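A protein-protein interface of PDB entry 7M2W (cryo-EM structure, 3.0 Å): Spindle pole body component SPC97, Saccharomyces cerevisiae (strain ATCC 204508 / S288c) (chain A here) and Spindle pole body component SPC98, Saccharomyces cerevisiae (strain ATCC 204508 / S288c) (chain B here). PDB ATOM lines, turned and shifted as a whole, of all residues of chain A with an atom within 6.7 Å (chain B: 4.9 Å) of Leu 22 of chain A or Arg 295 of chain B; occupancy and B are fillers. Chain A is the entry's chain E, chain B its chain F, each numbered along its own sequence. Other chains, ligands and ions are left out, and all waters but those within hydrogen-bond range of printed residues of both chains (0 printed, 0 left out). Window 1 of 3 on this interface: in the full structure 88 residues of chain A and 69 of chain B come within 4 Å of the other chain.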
ATOM      1  N   ILE A  19      14.437  25.672 -16.155  1.00  0.00           N
ATOM      2  CA  ILE A  19      13.222  25.597 -16.961  1.00  0.00           C
ATOM      3  C   ILE A  19      13.455  26.396 -18.235  1.00  0.00           C
ATOM      4  O   ILE A  19      13.911  27.543 -18.156  1.00  0.00           O
ATOM      5  CB  ILE A  19      11.998  26.135 -16.199  1.00  0.00           C
ATOM      6  CG1 ILE A  19      11.508  25.105 -15.188  1.00  0.00           C
ATOM      7  CG2 ILE A  19      10.880  26.475 -17.153  1.00  0.00           C
ATOM      8  CD1 ILE A  19      10.306  25.557 -14.411  1.00  0.00           C
ATOM      9  N   PRO A  20      13.175  25.840 -19.412  1.00  0.00           N
ATOM     10  CA  PRO A  20      13.396  26.587 -20.653  1.00  0.00           C
ATOM     11  C   PRO A  20      12.475  27.795 -20.749  1.00  0.00           C
ATOM     12  O   PRO A  20      11.659  28.055 -19.864  1.00  0.00           O
ATOM     13  CB  PRO A  20      13.088  25.559 -21.743  1.00  0.00           C
ATOM     14  CG  PRO A  20      13.270  24.243 -21.076  1.00  0.00           C
ATOM     15  CD  PRO A  20      12.790  24.447 -19.677  1.00  0.00           C
ATOM     16  N   LEU A  21      12.616  28.541 -21.845  1.00  0.00           N
ATOM     17  CA  LEU A  21      11.850  29.774 -22.003  1.00  0.00           C
ATOM     18  C   LEU A  21      10.351  29.500 -22.039  1.00  0.00           C
ATOM     19  O   LEU A  21       9.547  30.358 -21.661  1.00  0.00           O
ATOM     20  CB  LEU A  21      12.293  30.503 -23.270  1.00  0.00           C
ATOM     21  CG  LEU A  21      11.691  31.885 -23.509  1.00  0.00           C
ATOM     22  CD1 LEU A  21      11.808  32.721 -22.260  1.00  0.00           C
ATOM     23  CD2 LEU A  21      12.392  32.566 -24.656  1.00  0.00           C
ATOM     24  N   LEU A  22       9.956  28.308 -22.479  1.00  0.00           N
ATOM     25  CA  LEU A  22       8.553  27.936 -22.581  1.00  0.00           C
ATOM     26  C   LEU A  22       8.197  26.740 -21.711  1.00  0.00           C
ATOM     27  O   LEU A  22       7.136  26.139 -21.903  1.00  0.00           O
ATOM     28  CB  LEU A  22       8.187  27.656 -24.038  1.00  0.00           C
ATOM     29  CG  LEU A  22       8.321  28.868 -24.950  1.00  0.00           C
ATOM     30  CD1 LEU A  22       7.747  28.578 -26.307  1.00  0.00           C
ATOM     31  CD2 LEU A  22       7.610  30.035 -24.325  1.00  0.00           C
ATOM     32  N   GLY A  23       9.056  26.379 -20.768  1.00  0.00           N
ATOM     33  CA  GLY A  23       8.754  25.272 -19.894  1.00  0.00           C
ATOM     34  C   GLY A  23       7.569  25.563 -18.998  1.00  0.00           C
ATOM     35  O   GLY A  23       7.251  26.710 -18.688  1.00  0.00           O
ATOM     36  N   LYS A  24       6.900  24.494 -18.578  1.00  0.00           N
ATOM     37  CA  LYS A  24       5.714  24.639 -17.747  1.00  0.00           C
ATOM     38  C   LYS A  24       6.094  25.226 -16.396  1.00  0.00           C
ATOM     39  O   LYS A  24       6.981  24.714 -15.709  1.00  0.00           O
ATOM     40  CB  LYS A  24       5.029  23.285 -17.573  1.00  0.00           C
ATOM     41  CG  LYS A  24       3.683  23.351 -16.883  1.00  0.00           C
ATOM     42  CD  LYS A  24       2.815  22.161 -17.248  1.00  0.00           C
ATOM     43  CE  LYS A  24       3.558  20.853 -17.066  1.00  0.00           C
ATOM     44  NZ  LYS A  24       4.098  20.711 -15.689  1.00  0.00           N
ATOM     45  N   LEU A  25       5.419  26.309 -16.018  1.00  0.00           N
ATOM     46  CA  LEU A  25       5.734  27.038 -14.798  1.00  0.00           C
ATOM     47  C   LEU A  25       4.852  26.631 -13.629  1.00  0.00           C
ATOM     48  O   LEU A  25       5.174  26.956 -12.484  1.00  0.00           O
ATOM     49  CB  LEU A  25       5.624  28.543 -15.040  1.00  0.00           C
ATOM     50  CG  LEU A  25       6.704  29.155 -15.931  1.00  0.00           C
ATOM     51  CD1 LEU A  25       6.352  30.578 -16.301  1.00  0.00           C
ATOM     52  CD2 LEU A  25       8.047  29.098 -15.251  1.00  0.00           C
ATOM     53  N   VAL A  26       3.758  25.924 -13.885  1.00  0.00           N
ATOM     54  CA  VAL A  26       2.853  25.462 -12.843  1.00  0.00           C
ATOM     55  C   VAL A  26       3.280  24.061 -12.437  1.00  0.00           C
ATOM     56  O   VAL A  26       3.838  23.313 -13.246  1.00  0.00           O
ATOM     57  CB  VAL A  26       1.383  25.491 -13.312  1.00  0.00           C
ATOM     58  CG1 VAL A  26       1.100  24.356 -14.275  1.00  0.00           C
ATOM     59  CG2 VAL A  26       0.440  25.436 -12.132  1.00  0.00           C
ATOM     60  N   THR A 120       5.266  17.832 -26.643  1.00  0.00           N
ATOM     61  CA  THR A 120       5.104  19.024 -25.818  1.00  0.00           C
ATOM     62  C   THR A 120       6.386  19.335 -25.062  1.00  0.00           C
ATOM     63  O   THR A 120       6.883  20.471 -25.080  1.00  0.00           O
ATOM     64  CB  THR A 120       3.936  18.840 -24.850  1.00  0.00           C
ATOM     65  OG1 THR A 120       2.719  18.695 -25.586  1.00  0.00           O
ATOM     66  CG2 THR A 120       3.823  20.030 -23.928  1.00  0.00           C
ATOM     67  N   TYR A 123       9.050  20.709 -27.604  1.00  0.00           N
ATOM     68  CA  TYR A 123       8.982  22.111 -27.994  1.00  0.00           C
ATOM     69  C   TYR A 123       9.320  23.016 -26.816  1.00  0.00           C
ATOM     70  O   TYR A 123       9.994  24.039 -26.998  1.00  0.00           O
ATOM     71  CB  TYR A 123       7.619  22.461 -28.611  1.00  0.00           C
ATOM     72  CG  TYR A 123       6.489  22.825 -27.668  1.00  0.00           C
ATOM     73  CD1 TYR A 123       5.432  21.960 -27.464  1.00  0.00           C
ATOM     74  CD2 TYR A 123       6.451  24.056 -27.031  1.00  0.00           C
ATOM     75  CE1 TYR A 123       4.392  22.293 -26.624  1.00  0.00           C
ATOM     76  CE2 TYR A 123       5.423  24.389 -26.183  1.00  0.00           C
ATOM     77  CZ  TYR A 123       4.394  23.506 -25.987  1.00  0.00           C
ATOM     78  OH  TYR A 123       3.357  23.838 -25.148  1.00  0.00           O
ATOM     79  N   GLU A 124       8.891  22.647 -25.603  1.00  0.00           N
ATOM     80  CA  GLU A 124       9.337  23.386 -24.426  1.00  0.00           C
ATOM     81  C   GLU A 124      10.857  23.438 -24.355  1.00  0.00           C
ATOM     82  O   GLU A 124      11.436  24.508 -24.150  1.00  0.00           O
ATOM     83  CB  GLU A 124       8.768  22.762 -23.153  1.00  0.00           C
ATOM     84  CG  GLU A 124       7.269  22.921 -22.994  1.00  0.00           C
ATOM     85  CD  GLU A 124       6.760  22.341 -21.692  1.00  0.00           C
ATOM     86  OE1 GLU A 124       7.576  22.121 -20.775  1.00  0.00           O
ATOM     87  OE2 GLU A 124       5.539  22.106 -21.584  1.00  0.00           O
ATOM     88  N   LYS A 125      11.521  22.297 -24.553  1.00  0.00           N
ATOM     89  CA  LYS A 125      12.975  22.250 -24.433  1.00  0.00           C
ATOM     90  C   LYS A 125      13.655  23.058 -25.530  1.00  0.00           C
ATOM     91  O   LYS A 125      14.520  23.894 -25.248  1.00  0.00           O
ATOM     92  CB  LYS A 125      13.454  20.801 -24.465  1.00  0.00           C
ATOM     93  CG  LYS A 125      14.959  20.650 -24.396  1.00  0.00           C
ATOM     94  CD  LYS A 125      15.352  19.228 -24.043  1.00  0.00           C
ATOM     95  CE  LYS A 125      16.776  19.166 -23.519  1.00  0.00           C
ATOM     96  NZ  LYS A 125      16.969  18.028 -22.579  1.00  0.00           N
ATOM     97  N   SER A 127      12.591  25.445 -27.255  1.00  0.00           N
ATOM     98  CA  SER A 127      12.301  26.871 -27.268  1.00  0.00           C
ATOM     99  C   SER A 127      13.424  27.714 -26.681  1.00  0.00           C
ATOM    100  O   SER A 127      13.317  28.943 -26.685  1.00  0.00           O
ATOM    101  CB  SER A 127      11.008  27.148 -26.507  1.00  0.00           C
ATOM    102  OG  SER A 127      11.059  26.586 -25.211  1.00  0.00           O
ATOM    103  N   ASP A 128      14.490  27.093 -26.183  1.00  0.00           N
ATOM    104  CA  ASP A 128      15.591  27.820 -25.574  1.00  0.00           C
ATOM    105  C   ASP A 128      16.452  28.474 -26.654  1.00  0.00           C
ATOM    106  O   ASP A 128      16.230  28.302 -27.854  1.00  0.00           O
ATOM    107  CB  ASP A 128      16.412  26.885 -24.692  1.00  0.00           C
ATOM    108  CG  ASP A 128      17.063  27.603 -23.531  1.00  0.00           C
ATOM    109  OD1 ASP A 128      17.057  28.852 -23.523  1.00  0.00           O
ATOM    110  OD2 ASP A 128      17.568  26.920 -22.617  1.00  0.00           O
ATOM    111  N   ARG A 143       4.536  23.036 -31.662  1.00  0.00           N
ATOM    112  CA  ARG A 143       3.511  23.589 -30.783  1.00  0.00           C
ATOM    113  C   ARG A 143       2.291  24.028 -31.573  1.00  0.00           C
ATOM    114  O   ARG A 143       1.153  23.766 -31.172  1.00  0.00           O
ATOM    115  CB  ARG A 143       4.055  24.768 -29.988  1.00  0.00           C
ATOM    116  CG  ARG A 143       3.036  25.291 -29.004  1.00  0.00           C
ATOM    117  CD  ARG A 143       3.553  26.445 -28.186  1.00  0.00           C
ATOM    118  NE  ARG A 143       3.736  27.653 -28.975  1.00  0.00           N
ATOM    119  CZ  ARG A 143       4.920  28.183 -29.242  1.00  0.00           C
ATOM    120  NH1 ARG A 143       6.021  27.594 -28.802  1.00  0.00           N
ATOM    121  NH2 ARG A 143       5.006  29.293 -29.957  1.00  0.00           N
ATOM    122  N   GLU B 226      -2.436  27.566 -14.740  1.00  0.00           N
ATOM    123  CA  GLU B 226      -1.163  28.199 -15.050  1.00  0.00           C
ATOM    124  C   GLU B 226      -1.383  29.624 -15.534  1.00  0.00           C
ATOM    125  O   GLU B 226      -0.638  30.534 -15.162  1.00  0.00           O
ATOM    126  CB  GLU B 226      -0.404  27.386 -16.094  1.00  0.00           C
ATOM    127  CG  GLU B 226       0.938  27.981 -16.467  1.00  0.00           C
ATOM    128  CD  GLU B 226       1.738  27.081 -17.378  1.00  0.00           C
ATOM    129  OE1 GLU B 226       1.188  26.057 -17.832  1.00  0.00           O
ATOM    130  OE2 GLU B 226       2.910  27.401 -17.651  1.00  0.00           O
ATOM    131  N   LEU B 230      -0.033  32.928 -13.613  1.00  0.00           N
ATOM    132  CA  LEU B 230       0.834  33.835 -14.357  1.00  0.00           C
ATOM    133  C   LEU B 230       0.246  35.237 -14.404  1.00  0.00           C
ATOM    134  O   LEU B 230       0.976  36.227 -14.294  1.00  0.00           O
ATOM    135  CB  LEU B 230       1.059  33.300 -15.769  1.00  0.00           C
ATOM    136  CG  LEU B 230       1.976  32.091 -15.904  1.00  0.00           C
ATOM    137  CD1 LEU B 230       2.188  31.762 -17.364  1.00  0.00           C
ATOM    138  CD2 LEU B 230       3.295  32.335 -15.203  1.00  0.00           C
ATOM    139  N   ASN B 290      -2.464  31.897 -25.127  1.00  0.00           N
ATOM    140  CA  ASN B 290      -2.393  32.950 -24.123  1.00  0.00           C
ATOM    141  C   ASN B 290      -1.587  32.509 -22.911  1.00  0.00           C
ATOM    142  O   ASN B 290      -0.846  33.316 -22.339  1.00  0.00           O
ATOM    143  CB  ASN B 290      -3.796  33.389 -23.718  1.00  0.00           C
ATOM    144  CG  ASN B 290      -4.439  34.277 -24.754  1.00  0.00           C
ATOM    145  OD1 ASN B 290      -4.541  35.489 -24.572  1.00  0.00           O
ATOM    146  ND2 ASN B 290      -4.863  33.683 -25.858  1.00  0.00           N
ATOM    147  N   ILE B 291      -1.702  31.240 -22.515  1.00  0.00           N
ATOM    148  CA  ILE B 291      -0.810  30.709 -21.489  1.00  0.00           C
ATOM    149  C   ILE B 291       0.636  30.847 -21.934  1.00  0.00           C
ATOM    150  O   ILE B 291       1.510  31.216 -21.146  1.00  0.00           O
ATOM    151  CB  ILE B 291      -1.159  29.246 -21.169  1.00  0.00           C
ATOM    152  CG1 ILE B 291      -2.500  29.154 -20.454  1.00  0.00           C
ATOM    153  CG2 ILE B 291      -0.087  28.622 -20.303  1.00  0.00           C
ATOM    154  CD1 ILE B 291      -2.983  27.742 -20.271  1.00  0.00           C
ATOM    155  N   ILE B 292       0.907  30.586 -23.213  1.00  0.00           N
ATOM    156  CA  ILE B 292       2.279  30.664 -23.711  1.00  0.00           C
ATOM    157  C   ILE B 292       2.785  32.103 -23.681  1.00  0.00           C
ATOM    158  O   ILE B 292       3.927  32.370 -23.287  1.00  0.00           O
ATOM    159  CB  ILE B 292       2.372  30.057 -25.121  1.00  0.00           C
ATOM    160  CG1 ILE B 292       2.442  28.537 -25.025  1.00  0.00           C
ATOM    161  CG2 ILE B 292       3.587  30.582 -25.852  1.00  0.00           C
ATOM    162  CD1 ILE B 292       3.711  28.041 -24.399  1.00  0.00           C
ATOM    163  N   ARG B 293       1.952  33.049 -24.114  1.00  0.00           N
ATOM    164  CA  ARG B 293       2.353  34.452 -24.098  1.00  0.00           C
ATOM    165  C   ARG B 293       2.594  34.944 -22.678  1.00  0.00           C
ATOM    166  O   ARG B 293       3.551  35.685 -22.426  1.00  0.00           O
ATOM    167  CB  ARG B 293       1.300  35.311 -24.793  1.00  0.00           C
ATOM    168  CG  ARG B 293       1.139  35.008 -26.264  1.00  0.00           C
ATOM    169  CD  ARG B 293       0.090  35.902 -26.883  1.00  0.00           C
ATOM    170  NE  ARG B 293       0.362  37.303 -26.594  1.00  0.00           N
ATOM    171  CZ  ARG B 293       1.069  38.105 -27.382  1.00  0.00           C
ATOM    172  NH1 ARG B 293       1.577  37.646 -28.515  1.00  0.00           N
ATOM    173  NH2 ARG B 293       1.266  39.367 -27.036  1.00  0.00           N
ATOM    174  N   LEU B 294       1.739  34.548 -21.734  1.00  0.00           N
ATOM    175  CA  LEU B 294       1.961  34.932 -20.344  1.00  0.00           C
ATOM    176  C   LEU B 294       3.221  34.281 -19.795  1.00  0.00           C
ATOM    177  O   LEU B 294       3.924  34.872 -18.970  1.00  0.00           O
ATOM    178  CB  LEU B 294       0.753  34.558 -19.492  1.00  0.00           C
ATOM    179  CG  LEU B 294      -0.482  35.431 -19.676  1.00  0.00           C
ATOM    180  CD1 LEU B 294      -1.530  35.057 -18.657  1.00  0.00           C
ATOM    181  CD2 LEU B 294      -0.132  36.899 -19.576  1.00  0.00           C
ATOM    182  N   ARG B 295       3.525  33.069 -20.253  1.00  0.00           N
ATOM    183  CA  ARG B 295       4.764  32.409 -19.871  1.00  0.00           C
ATOM    184  C   ARG B 295       5.970  33.217 -20.327  1.00  0.00           C
ATOM    185  O   ARG B 295       6.889  33.482 -19.542  1.00  0.00           O
ATOM    186  CB  ARG B 295       4.785  31.013 -20.486  1.00  0.00           C
ATOM    187  CG  ARG B 295       5.584  29.990 -19.747  1.00  0.00           C
ATOM    188  CD  ARG B 295       5.443  28.658 -20.442  1.00  0.00           C
ATOM    189  NE  ARG B 295       4.226  27.965 -20.044  1.00  0.00           N
ATOM    190  CZ  ARG B 295       3.782  26.858 -20.625  1.00  0.00           C
ATOM    191  NH1 ARG B 295       4.455  26.323 -21.633  1.00  0.00           N
ATOM    192  NH2 ARG B 295       2.665  26.287 -20.206  1.00  0.00           N
ATOM    193  N   ILE B 296       5.976  33.619 -21.597  1.00  0.00           N
ATOM    194  CA  ILE B 296       7.056  34.444 -22.131  1.00  0.00           C
ATOM    195  C   ILE B 296       7.174  35.740 -21.343  1.00  0.00           C
ATOM    196  O   ILE B 296       8.274  36.161 -20.973  1.00  0.00           O
ATOM    197  CB  ILE B 296       6.824  34.730 -23.623  1.00  0.00           C
ATOM    198  CG1 ILE B 296       7.029  33.473 -24.452  1.00  0.00           C
ATOM    199  CG2 ILE B 296       7.752  35.822 -24.099  1.00  0.00           C
ATOM    200  CD1 ILE B 296       6.243  33.478 -25.729  1.00  0.00           C
ATOM    201  N   TYR B 297       6.044  36.405 -21.097  1.00  0.00           N
ATOM    202  CA  TYR B 297       6.078  37.684 -20.397  1.00  0.00           C
ATOM    203  C   TYR B 297       6.596  37.528 -18.973  1.00  0.00           C
ATOM    204  O   TYR B 297       7.286  38.413 -18.459  1.00  0.00           O
ATOM    205  CB  TYR B 297       4.689  38.313 -20.399  1.00  0.00           C
ATOM    206  CG  TYR B 297       4.469  39.299 -21.517  1.00  0.00           C
ATOM    207  CD1 TYR B 297       3.741  38.951 -22.639  1.00  0.00           C
ATOM    208  CD2 TYR B 297       4.979  40.583 -21.444  1.00  0.00           C
ATOM    209  CE1 TYR B 297       3.535  39.849 -23.662  1.00  0.00           C
ATOM    210  CE2 TYR B 297       4.774  41.488 -22.459  1.00  0.00           C
ATOM    211  CZ  TYR B 297       4.050  41.117 -23.565  1.00  0.00           C
ATOM    212  OH  TYR B 297       3.845  42.017 -24.583  1.00  0.00           O
ATOM    213  N   CYS B 298       6.273  36.416 -18.315  1.00  0.00           N
ATOM    214  CA  CYS B 298       6.744  36.207 -16.953  1.00  0.00           C
ATOM    215  C   CYS B 298       8.196  35.764 -16.900  1.00  0.00           C
ATOM    216  O   CYS B 298       8.847  35.963 -15.871  1.00  0.00           O
ATOM    217  CB  CYS B 298       5.859  35.182 -16.244  1.00  0.00           C
ATOM    218  SG  CYS B 298       6.362  34.767 -14.558  1.00  0.00           S
ATOM    219  N   ARG B 299       8.720  35.178 -17.975  1.00  0.00           N
ATOM    220  CA  ARG B 299      10.138  34.843 -18.043  1.00  0.00           C
ATOM    221  C   ARG B 299      11.008  36.038 -18.396  1.00  0.00           C
ATOM    222  O   ARG B 299      12.075  36.220 -17.802  1.00  0.00           O
ATOM    223  CB  ARG B 299      10.384  33.732 -19.064  1.00  0.00           C
ATOM    224  CG  ARG B 299       9.678  32.437 -18.761  1.00  0.00           C
ATOM    225  CD  ARG B 299       9.951  31.995 -17.347  1.00  0.00           C
ATOM    226  NE  ARG B 299      11.360  31.684 -17.155  1.00  0.00           N
ATOM    227  CZ  ARG B 299      11.919  30.535 -17.508  1.00  0.00           C
ATOM    228  NH1 ARG B 299      11.186  29.590 -18.073  1.00  0.00           N
ATOM    229  NH2 ARG B 299      13.210  30.333 -17.300  1.00  0.00           N
ATOM    230  N   ASP B 324      10.936  30.986 -32.880  1.00  0.00           N
ATOM    231  CA  ASP B 324       9.524  30.961 -32.523  1.00  0.00           C
ATOM    232  C   ASP B 324       8.920  32.316 -32.860  1.00  0.00           C
ATOM    233  O   ASP B 324       9.495  33.354 -32.522  1.00  0.00           O
ATOM    234  CB  ASP B 324       9.371  30.637 -31.038  1.00  0.00           C
ATOM    235  CG  ASP B 324       7.921  30.510 -30.595  1.00  0.00           C
ATOM    236  OD1 ASP B 324       7.049  31.243 -31.101  1.00  0.00           O
ATOM    237  OD2 ASP B 324       7.653  29.667 -29.716  1.00  0.00           O
ATOM    238  N   ILE B 327       7.578  34.294 -29.348  1.00  0.00           N
ATOM    239  CA  ILE B 327       8.665  34.914 -28.601  1.00  0.00           C
ATOM    240  C   ILE B 327       9.247  36.074 -29.390  1.00  0.00           C
ATOM    241  O   ILE B 327       9.524  37.145 -28.840  1.00  0.00           O
ATOM    242  CB  ILE B 327       9.748  33.877 -28.263  1.00  0.00           C
ATOM    243  CG1 ILE B 327       9.128  32.663 -27.583  1.00  0.00           C
ATOM    244  CG2 ILE B 327      10.804  34.496 -27.377  1.00  0.00           C
ATOM    245  CD1 ILE B 327      10.115  31.585 -27.264  1.00  0.00           C
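The backbone carbonyl oxygen (O) of Pro 20 of chain A is in hydrogen-bond range of the guanidinium group (NH1) of Arg 299 of chain B, 2.4 Å away.
The backbone carbonyl oxygen of Leu 22 of chain A is in hydrogen-bond range of the guanidinium group of Arg 295 of chain B (2.7 Å).
The backbone carbonyl oxygen (O) of Ile 19 of chain A is in hydrogen-bond range of the guanidinium group (NH2) of Arg 299 of chain B (3.0 Å).
NH2 of Arg 143 of chain A lies within salt-bridge range of OD2 of Asp 324 of chain B (2.7 Å).
OE2 of Glu 226 of chain B sits at hydrogen-bond distance from N of Leu 25 of chain A (3.2 Å).
The backbone NH of Leu 22 of chain A sits close to the side-chain hydroxyl of Ser 127 of chain A.
OE2 of Glu 226 of chain B is in salt-bridge range of NE of Arg 295 of chain B, 2.8 Å away.
The side-chain carboxylate (OE1) of Glu 124 of chain A is in hydrogen-bond range of the backbone NH (N) of Lys 24 of chain A (3.3 Å).
Among the printed residues, pairs that only touch across the chains: Gly 23 of chain A with Arg 295 of chain B (3.2 Å), Leu 22 of chain A with Ile 296 of chain B (3.5 Å), Leu 21 of chain A with Arg 299 of chain B (3.6 Å), Leu 25 of chain A with Arg 295 of chain B (3.6 Å), Leu 22 of chain A with Asp 324 of chain B (3.6 Å), Leu 21 of chain A with Ile 327 of chain B (3.6 Å), Leu 25 of chain A with Leu 230 of chain B (3.7 Å), Lys 24 of chain A with Glu 226 of chain B (3.8 Å), Val 26 of chain A with Glu 226 of chain B (3.8 Å), Leu 22 of chain A with Ile 327 of chain B (3.9 Å) and Arg 143 of chain A with Ile 292 of chain B (3.95 Å).
Of chain B, only Arg 295, Ile 296, Asp 324 and Ile 327 come within 4 Å of Leu 22 of chain A.
Of chain A, only Leu 22, Gly 23 and Leu 25 come within 4 Å of Arg 295 of chain B.
Printed residues of chain B within 4 Å of Val 26 of chain A: Glu 226 (3.8 Å).
Printed residues of chain A within 4 Å of Ile 292 of chain B: Arg 143 (3.95 Å).
Of the printed residues of chain A, Arg 299 of chain B touches Ile 19 (3.0 Å), Pro 20 (2.4 Å) and Leu 21 (3.6 Å).
Asp 128 of chain A touches none of the printed residues of chain B.
Lys 125 of chain A touches none of the printed residues of chain B.
The nearest residue of chain B that does not touch Leu 22 of chain A is Ile 292 of chain B (4.3 Å).
Hydrophobic or aromatic side chains of chain B that line the printed part of chain A: Leu 230, Ile 292, Ile 296 and Ile 327.
Hydrophobic or aromatic side chains of chain A within 4 Å of the printed part of chain B: Ile 19, Leu 21, Leu 22, Leu 25 and Val 26.
Among the printed residues, 16 pairs touch across the chains.
Among the printed residues, Asp or Glu carboxylates within 4 Å of a Lys or Arg side-chain nitrogen of the other chain: Arg 143 of chain A with Asp 324 of chain B (2.7 Å).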
